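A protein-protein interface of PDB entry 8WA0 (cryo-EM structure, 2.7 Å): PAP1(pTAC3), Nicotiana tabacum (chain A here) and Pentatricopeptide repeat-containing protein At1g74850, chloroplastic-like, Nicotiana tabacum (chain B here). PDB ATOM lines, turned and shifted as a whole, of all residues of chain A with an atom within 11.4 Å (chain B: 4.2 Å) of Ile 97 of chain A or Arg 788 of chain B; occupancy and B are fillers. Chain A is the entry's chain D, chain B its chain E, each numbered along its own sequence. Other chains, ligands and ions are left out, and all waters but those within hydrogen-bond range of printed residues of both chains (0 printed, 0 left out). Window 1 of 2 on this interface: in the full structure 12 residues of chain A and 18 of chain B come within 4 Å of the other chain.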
ATOM      1  N   GLU A  66      -2.556 -18.539  30.448  1.00  0.00           N
ATOM      2  CA  GLU A  66      -1.980 -18.397  29.132  1.00  0.00           C
ATOM      3  C   GLU A  66      -2.938 -17.610  28.331  1.00  0.00           C
ATOM      4  O   GLU A  66      -2.545 -16.785  27.538  1.00  0.00           O
ATOM      5  CB  GLU A  66      -1.793 -19.749  28.479  1.00  0.00           C
ATOM      6  N   LEU A  69      -2.758 -13.843  28.953  1.00  0.00           N
ATOM      7  CA  LEU A  69      -1.547 -13.302  28.341  1.00  0.00           C
ATOM      8  C   LEU A  69      -1.499 -13.384  26.821  1.00  0.00           C
ATOM      9  O   LEU A  69      -1.052 -12.457  26.157  1.00  0.00           O
ATOM     10  CB  LEU A  69      -0.272 -13.866  28.985  1.00  0.00           C
ATOM     11  N   PHE A  73      -1.049 -10.052  24.591  1.00  0.00           N
ATOM     12  CA  PHE A  73       0.044  -9.770  23.699  1.00  0.00           C
ATOM     13  C   PHE A  73      -0.466  -9.425  22.329  1.00  0.00           C
ATOM     14  O   PHE A  73      -0.073  -8.428  21.744  1.00  0.00           O
ATOM     15  CB  PHE A  73       0.952 -10.994  23.565  1.00  0.00           C
ATOM     16  N   GLY A  88       8.178  -2.824  14.742  1.00  0.00           N
ATOM     17  CA  GLY A  88       7.628  -2.945  16.060  1.00  0.00           C
ATOM     18  C   GLY A  88       7.308  -4.386  16.267  1.00  0.00           C
ATOM     19  O   GLY A  88       7.618  -4.970  17.298  1.00  0.00           O
ATOM     20  N   VAL A  89       6.747  -4.993  15.253  1.00  0.00           N
ATOM     21  CA  VAL A  89       6.325  -6.364  15.371  1.00  0.00           C
ATOM     22  C   VAL A  89       7.492  -7.234  15.633  1.00  0.00           C
ATOM     23  O   VAL A  89       7.400  -8.200  16.347  1.00  0.00           O
ATOM     24  CB  VAL A  89       5.638  -6.824  14.072  1.00  0.00           C
ATOM     25  N   SER A  90       8.603  -6.916  15.029  1.00  0.00           N
ATOM     26  CA  SER A  90       9.727  -7.798  15.157  1.00  0.00           C
ATOM     27  C   SER A  90      10.130  -7.910  16.605  1.00  0.00           C
ATOM     28  O   SER A  90      10.419  -9.002  17.073  1.00  0.00           O
ATOM     29  CB  SER A  90      10.899  -7.316  14.306  1.00  0.00           C
ATOM     30  N   GLN A  91      10.123  -6.795  17.332  1.00  0.00           N
ATOM     31  CA  GLN A  91      10.453  -6.859  18.736  1.00  0.00           C
ATOM     32  C   GLN A  91       9.427  -7.723  19.429  1.00  0.00           C
ATOM     33  O   GLN A  91       9.801  -8.624  20.138  1.00  0.00           O
ATOM     34  CB  GLN A  91      10.427  -5.481  19.334  1.00  0.00           C
ATOM     35  N   VAL A  92       8.145  -7.535  19.139  1.00  0.00           N
ATOM     36  CA  VAL A  92       7.113  -8.293  19.790  1.00  0.00           C
ATOM     37  C   VAL A  92       7.309  -9.717  19.457  1.00  0.00           C
ATOM     38  O   VAL A  92       7.095 -10.588  20.269  1.00  0.00           O
ATOM     39  CB  VAL A  92       5.738  -7.834  19.376  1.00  0.00           C
ATOM     40  N   ILE A  93       7.774  -9.980  18.245  1.00  0.00           N
ATOM     41  CA  ILE A  93       8.058 -11.352  17.838  1.00  0.00           C
ATOM     42  C   ILE A  93       9.178 -11.932  18.687  1.00  0.00           C
ATOM     43  O   ILE A  93       9.072 -13.051  19.173  1.00  0.00           O
ATOM     44  CB  ILE A  93       8.400 -11.439  16.335  1.00  0.00           C
ATOM     45  N   TYR A  94      10.258 -11.187  18.875  1.00  0.00           N
ATOM     46  CA  TYR A  94      11.305 -11.665  19.761  1.00  0.00           C
ATOM     47  C   TYR A  94      10.735 -11.760  21.161  1.00  0.00           C
ATOM     48  O   TYR A  94      11.029 -12.702  21.890  1.00  0.00           O
ATOM     49  CB  TYR A  94      12.510 -10.740  19.729  1.00  0.00           C
ATOM     50  N   ASP A  95       9.923 -10.780  21.543  1.00  0.00           N
ATOM     51  CA  ASP A  95       9.290 -10.809  22.845  1.00  0.00           C
ATOM     52  C   ASP A  95       8.590 -12.117  22.985  1.00  0.00           C
ATOM     53  O   ASP A  95       8.463 -12.640  24.090  1.00  0.00           O
ATOM     54  CB  ASP A  95       8.185  -9.764  22.951  1.00  0.00           C
ATOM     55  N   MET A  96       8.098 -12.651  21.875  1.00  0.00           N
ATOM     56  CA  MET A  96       7.324 -13.833  22.013  1.00  0.00           C
ATOM     57  C   MET A  96       8.195 -14.972  22.456  1.00  0.00           C
ATOM     58  O   MET A  96       7.762 -15.815  23.226  1.00  0.00           O
ATOM     59  CB  MET A  96       6.608 -14.156  20.700  1.00  0.00           C
ATOM     60  N   ILE A  97       9.411 -15.044  21.964  1.00  0.00           N
ATOM     61  CA  ILE A  97      10.173 -16.197  22.325  1.00  0.00           C
ATOM     62  C   ILE A  97      10.611 -16.113  23.760  1.00  0.00           C
ATOM     63  O   ILE A  97      11.056 -17.103  24.330  1.00  0.00           O
ATOM     64  CB  ILE A  97      11.291 -16.516  21.363  1.00  0.00           C
ATOM     65  N   ALA A  98      10.556 -14.907  24.304  1.00  0.00           N
ATOM     66  CA  ALA A  98      11.046 -14.685  25.656  1.00  0.00           C
ATOM     67  C   ALA A  98      10.040 -15.075  26.661  1.00  0.00           C
ATOM     68  O   ALA A  98      10.321 -15.845  27.555  1.00  0.00           O
ATOM     69  CB  ALA A  98      11.428 -13.226  25.844  1.00  0.00           C
ATOM     70  N   ALA A  99       8.832 -14.606  26.478  1.00  0.00           N
ATOM     71  CA  ALA A  99       7.771 -14.961  27.375  1.00  0.00           C
ATOM     72  C   ALA A  99       7.601 -16.434  27.257  1.00  0.00           C
ATOM     73  O   ALA A  99       7.070 -17.067  28.160  1.00  0.00           O
ATOM     74  CB  ALA A  99       6.493 -14.255  26.980  1.00  0.00           C
ATOM     75  N   GLY A 100       8.021 -16.993  26.126  1.00  0.00           N
ATOM     76  CA  GLY A 100       7.840 -18.410  25.884  1.00  0.00           C
ATOM     77  C   GLY A 100       6.495 -18.631  25.279  1.00  0.00           C
ATOM     78  O   GLY A 100       6.029 -19.761  25.159  1.00  0.00           O
ATOM     79  N   LEU A 101       5.856 -17.539  24.906  1.00  0.00           N
ATOM     80  CA  LEU A 101       4.587 -17.652  24.281  1.00  0.00           C
ATOM     81  C   LEU A 101       4.913 -18.404  23.019  1.00  0.00           C
ATOM     82  O   LEU A 101       5.896 -18.106  22.350  1.00  0.00           O
ATOM     83  CB  LEU A 101       4.068 -16.256  23.995  1.00  0.00           C
ATOM     84  N   SER A 102       4.102 -19.396  22.686  1.00  0.00           N
ATOM     85  CA  SER A 102       4.394 -20.226  21.524  1.00  0.00           C
ATOM     86  C   SER A 102       4.311 -19.452  20.229  1.00  0.00           C
ATOM     87  O   SER A 102       3.423 -18.619  20.057  1.00  0.00           O
ATOM     88  CB  SER A 102       3.428 -21.412  21.481  1.00  0.00           C
ATOM     89  N   PRO A 103       5.237 -19.724  19.298  1.00  0.00           N
ATOM     90  CA  PRO A 103       5.101 -19.073  17.994  1.00  0.00           C
ATOM     91  C   PRO A 103       3.819 -19.551  17.321  1.00  0.00           C
ATOM     92  O   PRO A 103       3.512 -20.742  17.367  1.00  0.00           O
ATOM     93  CB  PRO A 103       6.332 -19.555  17.223  1.00  0.00           C
ATOM     94  N   GLY A 104       3.083 -18.644  16.697  1.00  0.00           N
ATOM     95  CA  GLY A 104       1.825 -19.013  16.090  1.00  0.00           C
ATOM     96  C   GLY A 104       1.705 -18.607  14.639  1.00  0.00           C
ATOM     97  O   GLY A 104       2.261 -17.605  14.206  1.00  0.00           O
ATOM     98  N   SER A 107       0.209 -15.392  14.638  1.00  0.00           N
ATOM     99  CA  SER A 107       1.128 -14.346  15.034  1.00  0.00           C
ATOM    100  C   SER A 107       2.017 -13.890  13.903  1.00  0.00           C
ATOM    101  O   SER A 107       2.238 -12.698  13.717  1.00  0.00           O
ATOM    102  CB  SER A 107       1.982 -14.812  16.201  1.00  0.00           C
ATOM    103  N   PHE A 108       2.502 -14.823  13.115  1.00  0.00           N
ATOM    104  CA  PHE A 108       3.320 -14.465  11.994  1.00  0.00           C
ATOM    105  C   PHE A 108       2.530 -13.646  11.034  1.00  0.00           C
ATOM    106  O   PHE A 108       3.096 -12.880  10.273  1.00  0.00           O
ATOM    107  CB  PHE A 108       3.784 -15.723  11.272  1.00  0.00           C
ATOM    108  N   GLU A 134      10.083 -22.560  10.768  1.00  0.00           N
ATOM    109  CA  GLU A 134       9.570 -22.981  12.054  1.00  0.00           C
ATOM    110  C   GLU A 134       8.830 -24.290  11.849  1.00  0.00           C
ATOM    111  O   GLU A 134       8.935 -25.189  12.669  1.00  0.00           O
ATOM    112  CB  GLU A 134       8.635 -21.911  12.587  1.00  0.00           C
ATOM    113  N   SER B 744       9.113 -13.465  32.181  1.00  0.00           N
ATOM    114  CA  SER B 744       9.703 -14.765  31.908  1.00  0.00           C
ATOM    115  C   SER B 744      11.205 -14.739  32.159  1.00  0.00           C
ATOM    116  O   SER B 744      11.821 -13.680  32.293  1.00  0.00           O
ATOM    117  CB  SER B 744       9.425 -15.198  30.464  1.00  0.00           C
ATOM    118  OG  SER B 744       9.995 -16.467  30.192  1.00  0.00           O
ATOM    119  N   VAL B 745      11.788 -15.933  32.228  1.00  0.00           N
ATOM    120  CA  VAL B 745      13.229 -16.117  32.385  1.00  0.00           C
ATOM    121  C   VAL B 745      13.645 -17.160  31.357  1.00  0.00           C
ATOM    122  O   VAL B 745      13.494 -18.365  31.587  1.00  0.00           O
ATOM    123  CB  VAL B 745      13.619 -16.550  33.802  1.00  0.00           C
ATOM    124  CG1 VAL B 745      15.124 -16.759  33.897  1.00  0.00           C
ATOM    125  CG2 VAL B 745      13.159 -15.520  34.825  1.00  0.00           C
ATOM    126  N   VAL B 746      14.172 -16.706  30.221  1.00  0.00           N
ATOM    127  CA  VAL B 746      14.546 -17.597  29.125  1.00  0.00           C
ATOM    128  C   VAL B 746      15.838 -18.301  29.529  1.00  0.00           C
ATOM    129  O   VAL B 746      16.925 -17.727  29.445  1.00  0.00           O
ATOM    130  CB  VAL B 746      14.703 -16.843  27.803  1.00  0.00           C
ATOM    131  CG1 VAL B 746      14.958 -17.818  26.663  1.00  0.00           C
ATOM    132  CG2 VAL B 746      13.470 -15.997  27.526  1.00  0.00           C
ATOM    133  N   VAL B 747      15.724 -19.551  29.965  1.00  0.00           N
ATOM    134  CA  VAL B 747      16.868 -20.336  30.415  1.00  0.00           C
ATOM    135  C   VAL B 747      17.299 -21.353  29.366  1.00  0.00           C
ATOM    136  O   VAL B 747      18.490 -21.511  29.097  1.00  0.00           O
ATOM    137  CB  VAL B 747      16.552 -21.013  31.769  1.00  0.00           C
ATOM    138  CG1 VAL B 747      15.195 -21.703  31.726  1.00  0.00           C
ATOM    139  CG2 VAL B 747      17.650 -21.997  32.145  1.00  0.00           C
ATOM    140  N   VAL B 748      16.344 -22.049  28.754  1.00  0.00           N
ATOM    141  CA  VAL B 748      16.637 -23.074  27.757  1.00  0.00           C
ATOM    142  C   VAL B 748      15.667 -22.912  26.594  1.00  0.00           C
ATOM    143  O   VAL B 748      14.454 -22.792  26.799  1.00  0.00           O
ATOM    144  CB  VAL B 748      16.555 -24.495  28.351  1.00  0.00           C
ATOM    145  CG1 VAL B 748      15.288 -24.662  29.180  1.00  0.00           C
ATOM    146  CG2 VAL B 748      16.622 -25.543  27.250  1.00  0.00           C
ATOM    147  N   ARG B 749      16.179 -22.866  25.368  1.00  0.00           N
ATOM    148  CA  ARG B 749      15.413 -22.719  24.125  1.00  0.00           C
ATOM    149  C   ARG B 749      15.558 -23.921  23.260  1.00  0.00           C
ATOM    150  O   ARG B 749      16.076 -24.935  23.694  1.00  0.00           O
ATOM    151  CB  ARG B 749      15.983 -21.621  23.284  1.00  0.00           C
ATOM    152  CG  ARG B 749      14.997 -20.808  22.482  1.00  0.00           C
ATOM    153  CD  ARG B 749      15.475 -19.386  22.359  1.00  0.00           C
ATOM    154  NE  ARG B 749      14.858 -18.731  21.223  1.00  0.00           N
ATOM    155  CZ  ARG B 749      14.971 -17.437  20.974  1.00  0.00           C
ATOM    156  NH1 ARG B 749      14.382 -16.909  19.911  1.00  0.00           N
ATOM    157  NH2 ARG B 749      15.671 -16.668  21.792  1.00  0.00           N
ATOM    158  N   GLU B 753      12.443 -27.634  24.013  1.00  0.00           N
ATOM    159  CA  GLU B 753      11.671 -26.871  25.000  1.00  0.00           C
ATOM    160  C   GLU B 753      10.434 -27.530  25.500  1.00  0.00           C
ATOM    161  O   GLU B 753      10.111 -27.422  26.670  1.00  0.00           O
ATOM    162  CB  GLU B 753      11.225 -25.600  24.351  1.00  0.00           C
ATOM    163  CG  GLU B 753      12.071 -24.385  24.661  1.00  0.00           C
ATOM    164  CD  GLU B 753      11.649 -23.185  23.840  1.00  0.00           C
ATOM    165  OE1 GLU B 753      12.115 -22.066  24.124  1.00  0.00           O
ATOM    166  OE2 GLU B 753      10.839 -23.364  22.906  1.00  0.00           O
ATOM    167  N   PHE B 781       7.944 -23.426  36.216  1.00  0.00           N
ATOM    168  CA  PHE B 781       7.832 -23.726  34.782  1.00  0.00           C
ATOM    169  C   PHE B 781       6.418 -23.578  34.245  1.00  0.00           C
ATOM    170  O   PHE B 781       5.460 -24.016  34.877  1.00  0.00           O
ATOM    171  CB  PHE B 781       8.340 -25.137  34.472  1.00  0.00           C
ATOM    172  CG  PHE B 781       9.837 -25.255  34.462  1.00  0.00           C
ATOM    173  CD1 PHE B 781      10.536 -25.511  35.629  1.00  0.00           C
ATOM    174  CD2 PHE B 781      10.544 -25.121  33.281  1.00  0.00           C
ATOM    175  CE1 PHE B 781      11.913 -25.622  35.620  1.00  0.00           C
ATOM    176  CE2 PHE B 781      11.921 -25.229  33.264  1.00  0.00           C
ATOM    177  CZ  PHE B 781      12.607 -25.481  34.436  1.00  0.00           C
ATOM    178  N   PRO B 782       6.283 -22.961  33.064  1.00  0.00           N
ATOM    179  CA  PRO B 782       4.964 -22.768  32.453  1.00  0.00           C
ATOM    180  C   PRO B 782       4.359 -24.087  32.035  1.00  0.00           C
ATOM    181  O   PRO B 782       5.094 -25.025  31.731  1.00  0.00           O
ATOM    182  CB  PRO B 782       5.278 -21.956  31.196  1.00  0.00           C
ATOM    183  CG  PRO B 782       6.558 -21.266  31.494  1.00  0.00           C
ATOM    184  CD  PRO B 782       7.333 -22.212  32.358  1.00  0.00           C
ATOM    185  N   ASN B 785       4.895 -24.272  27.930  1.00  0.00           N
ATOM    186  CA  ASN B 785       6.267 -24.533  27.511  1.00  0.00           C
ATOM    187  C   ASN B 785       7.119 -24.709  28.755  1.00  0.00           C
ATOM    188  O   ASN B 785       7.266 -23.774  29.546  1.00  0.00           O
ATOM    189  CB  ASN B 785       6.810 -23.393  26.640  1.00  0.00           C
ATOM    190  CG  ASN B 785       8.101 -23.760  25.929  1.00  0.00           C
ATOM    191  OD1 ASN B 785       8.887 -24.572  26.418  1.00  0.00           O
ATOM    192  ND2 ASN B 785       8.324 -23.161  24.766  1.00  0.00           N
ATOM    193  N   LYS B 786       7.682 -25.904  28.924  1.00  0.00           N
ATOM    194  CA  LYS B 786       8.505 -26.216  30.092  1.00  0.00           C
ATOM    195  C   LYS B 786       9.980 -25.940  29.794  1.00  0.00           C
ATOM    196  O   LYS B 786      10.839 -26.817  29.868  1.00  0.00           O
ATOM    197  CB  LYS B 786       8.285 -27.664  30.518  1.00  0.00           C
ATOM    198  CG  LYS B 786       6.836 -28.009  30.815  1.00  0.00           C
ATOM    199  CD  LYS B 786       6.666 -29.497  31.072  1.00  0.00           C
ATOM    200  CE  LYS B 786       7.089 -30.315  29.862  1.00  0.00           C
ATOM    201  NZ  LYS B 786       6.925 -31.776  30.092  1.00  0.00           N
ATOM    202  N   GLY B 787      10.263 -24.687  29.453  1.00  0.00           N
ATOM    203  CA  GLY B 787      11.617 -24.299  29.111  1.00  0.00           C
ATOM    204  C   GLY B 787      12.017 -22.930  29.621  1.00  0.00           C
ATOM    205  O   GLY B 787      12.982 -22.339  29.131  1.00  0.00           O
ATOM    206  N   ARG B 788      11.288 -22.418  30.607  1.00  0.00           N
ATOM    207  CA  ARG B 788      11.572 -21.102  31.165  1.00  0.00           C
ATOM    208  C   ARG B 788      10.905 -21.000  32.531  1.00  0.00           C
ATOM    209  O   ARG B 788      10.329 -21.966  33.038  1.00  0.00           O
ATOM    210  CB  ARG B 788      11.106 -19.992  30.222  1.00  0.00           C
ATOM    211  CG  ARG B 788       9.765 -20.260  29.570  1.00  0.00           C
ATOM    212  CD  ARG B 788       9.527 -19.309  28.412  1.00  0.00           C
ATOM    213  NE  ARG B 788      10.726 -19.128  27.597  1.00  0.00           N
ATOM    214  CZ  ARG B 788      11.164 -20.002  26.695  1.00  0.00           C
ATOM    215  NH1 ARG B 788      10.508 -21.135  26.488  1.00  0.00           N
ATOM    216  NH2 ARG B 788      12.265 -19.745  26.002  1.00  0.00           N
ATOM    217  N   ILE B 789      11.001 -19.816  33.130  1.00  0.00           N
ATOM    218  CA  ILE B 789      10.403 -19.527  34.429  1.00  0.00           C
ATOM    219  C   ILE B 789       9.580 -18.256  34.271  1.00  0.00           C
ATOM    220  O   ILE B 789      10.133 -17.187  33.990  1.00  0.00           O
ATOM    221  CB  ILE B 789      11.454 -19.359  35.534  1.00  0.00           C
ATOM    222  CG1 ILE B 789      12.404 -20.559  35.565  1.00  0.00           C
ATOM    223  CG2 ILE B 789      10.777 -19.201  36.879  1.00  0.00           C
ATOM    224  CD1 ILE B 789      11.742 -21.846  35.995  1.00  0.00           C
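Ile 97 of chain A touches just these residues of chain B: Arg 749 and Arg 788. Of the printed residues of chain B, Ala 98 of chain A touches Ser 744, Val 746 and Arg 788. Of the printed residues of chain B, Gly 100 of chain A touches Asn 785 and Arg 788. Phe 108 of chain A touches none of the printed residues of chain B. Val 745 of chain B touches none of the printed residues of chain A. Of chain A, only Ile 97 comes within 4 Å of Arg 749 of chain B. No residue of chain A comes within 4 Å of Phe 781 of chain B. No residue of chain A comes within 4 Å of Pro 782 of chain B. Of chain A, only Ile 97 (3.4 Å), Ala 98 (3.3 Å), Ala 99 (3.3 Å) and Gly 100 (3.2 Å) come within 4 Å of Arg 788 of chain B. The nearest printed residue of chain B that does not touch Ile 97 of chain A is Val 746 of chain B (4.2 Å).
O of Glu 753 of chain B lies close to OD1 of Asn 785 of chain B, 3.1 Å away. The side-chain carboxylate (OE1) of Glu 753 of chain B lies within salt-bridge range of the guanidinium group (NH2) of Arg 788 of chain B (3.0 Å). The side-chain amide oxygen of Asn 785 of chain B lies close to the backbone NH of Gly 787 of chain B. The guanidinium group (NH1) of Arg 788 of chain B sits close to the side-chain amide nitrogen (ND2) of Asn 785 of chain B, 3.4 Å away.
Hydrophobic or aromatic side chains of chain A that line the printed part of chain B: Ile 97 and Ala 98. Among the printed residues, no Asp or Glu carboxylate lies within 4 Å of a Lys or Arg side-chain nitrogen of the other chain.
Among the printed residues, merely in contact across the chains: Ile 97 of chain A with Arg 749 of chain B (3.4 Å), Ala 98 of chain A with Val 746 of chain B (3.2 Å), Ala 99 of chain A with Ser 744 of chain B (3.5 Å), Ala 99 of chain A with Arg 788 of chain B (3.3 Å), Gly 100 of chain A with Asn 785 of chain B (3.999 Å) and Gly 100 of chain A with Arg 788 of chain B (3.2 Å).
The backbone carbonyl oxygen (O) of Ala 98 of chain A sits at hydrogen-bond distance from the guanidinium group (NE) of Arg 788 of chain B (3.3 Å). O of Ile 97 of chain A sits at hydrogen-bond distance from NH2 of Arg 788 of chain B, 3.4 Å away. The side-chain hydroxyl (OG) of Ser 744 of chain B sits at hydrogen-bond distance from the backbone carbonyl oxygen (O) of Ala 98 of chain A (2.7 Å).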
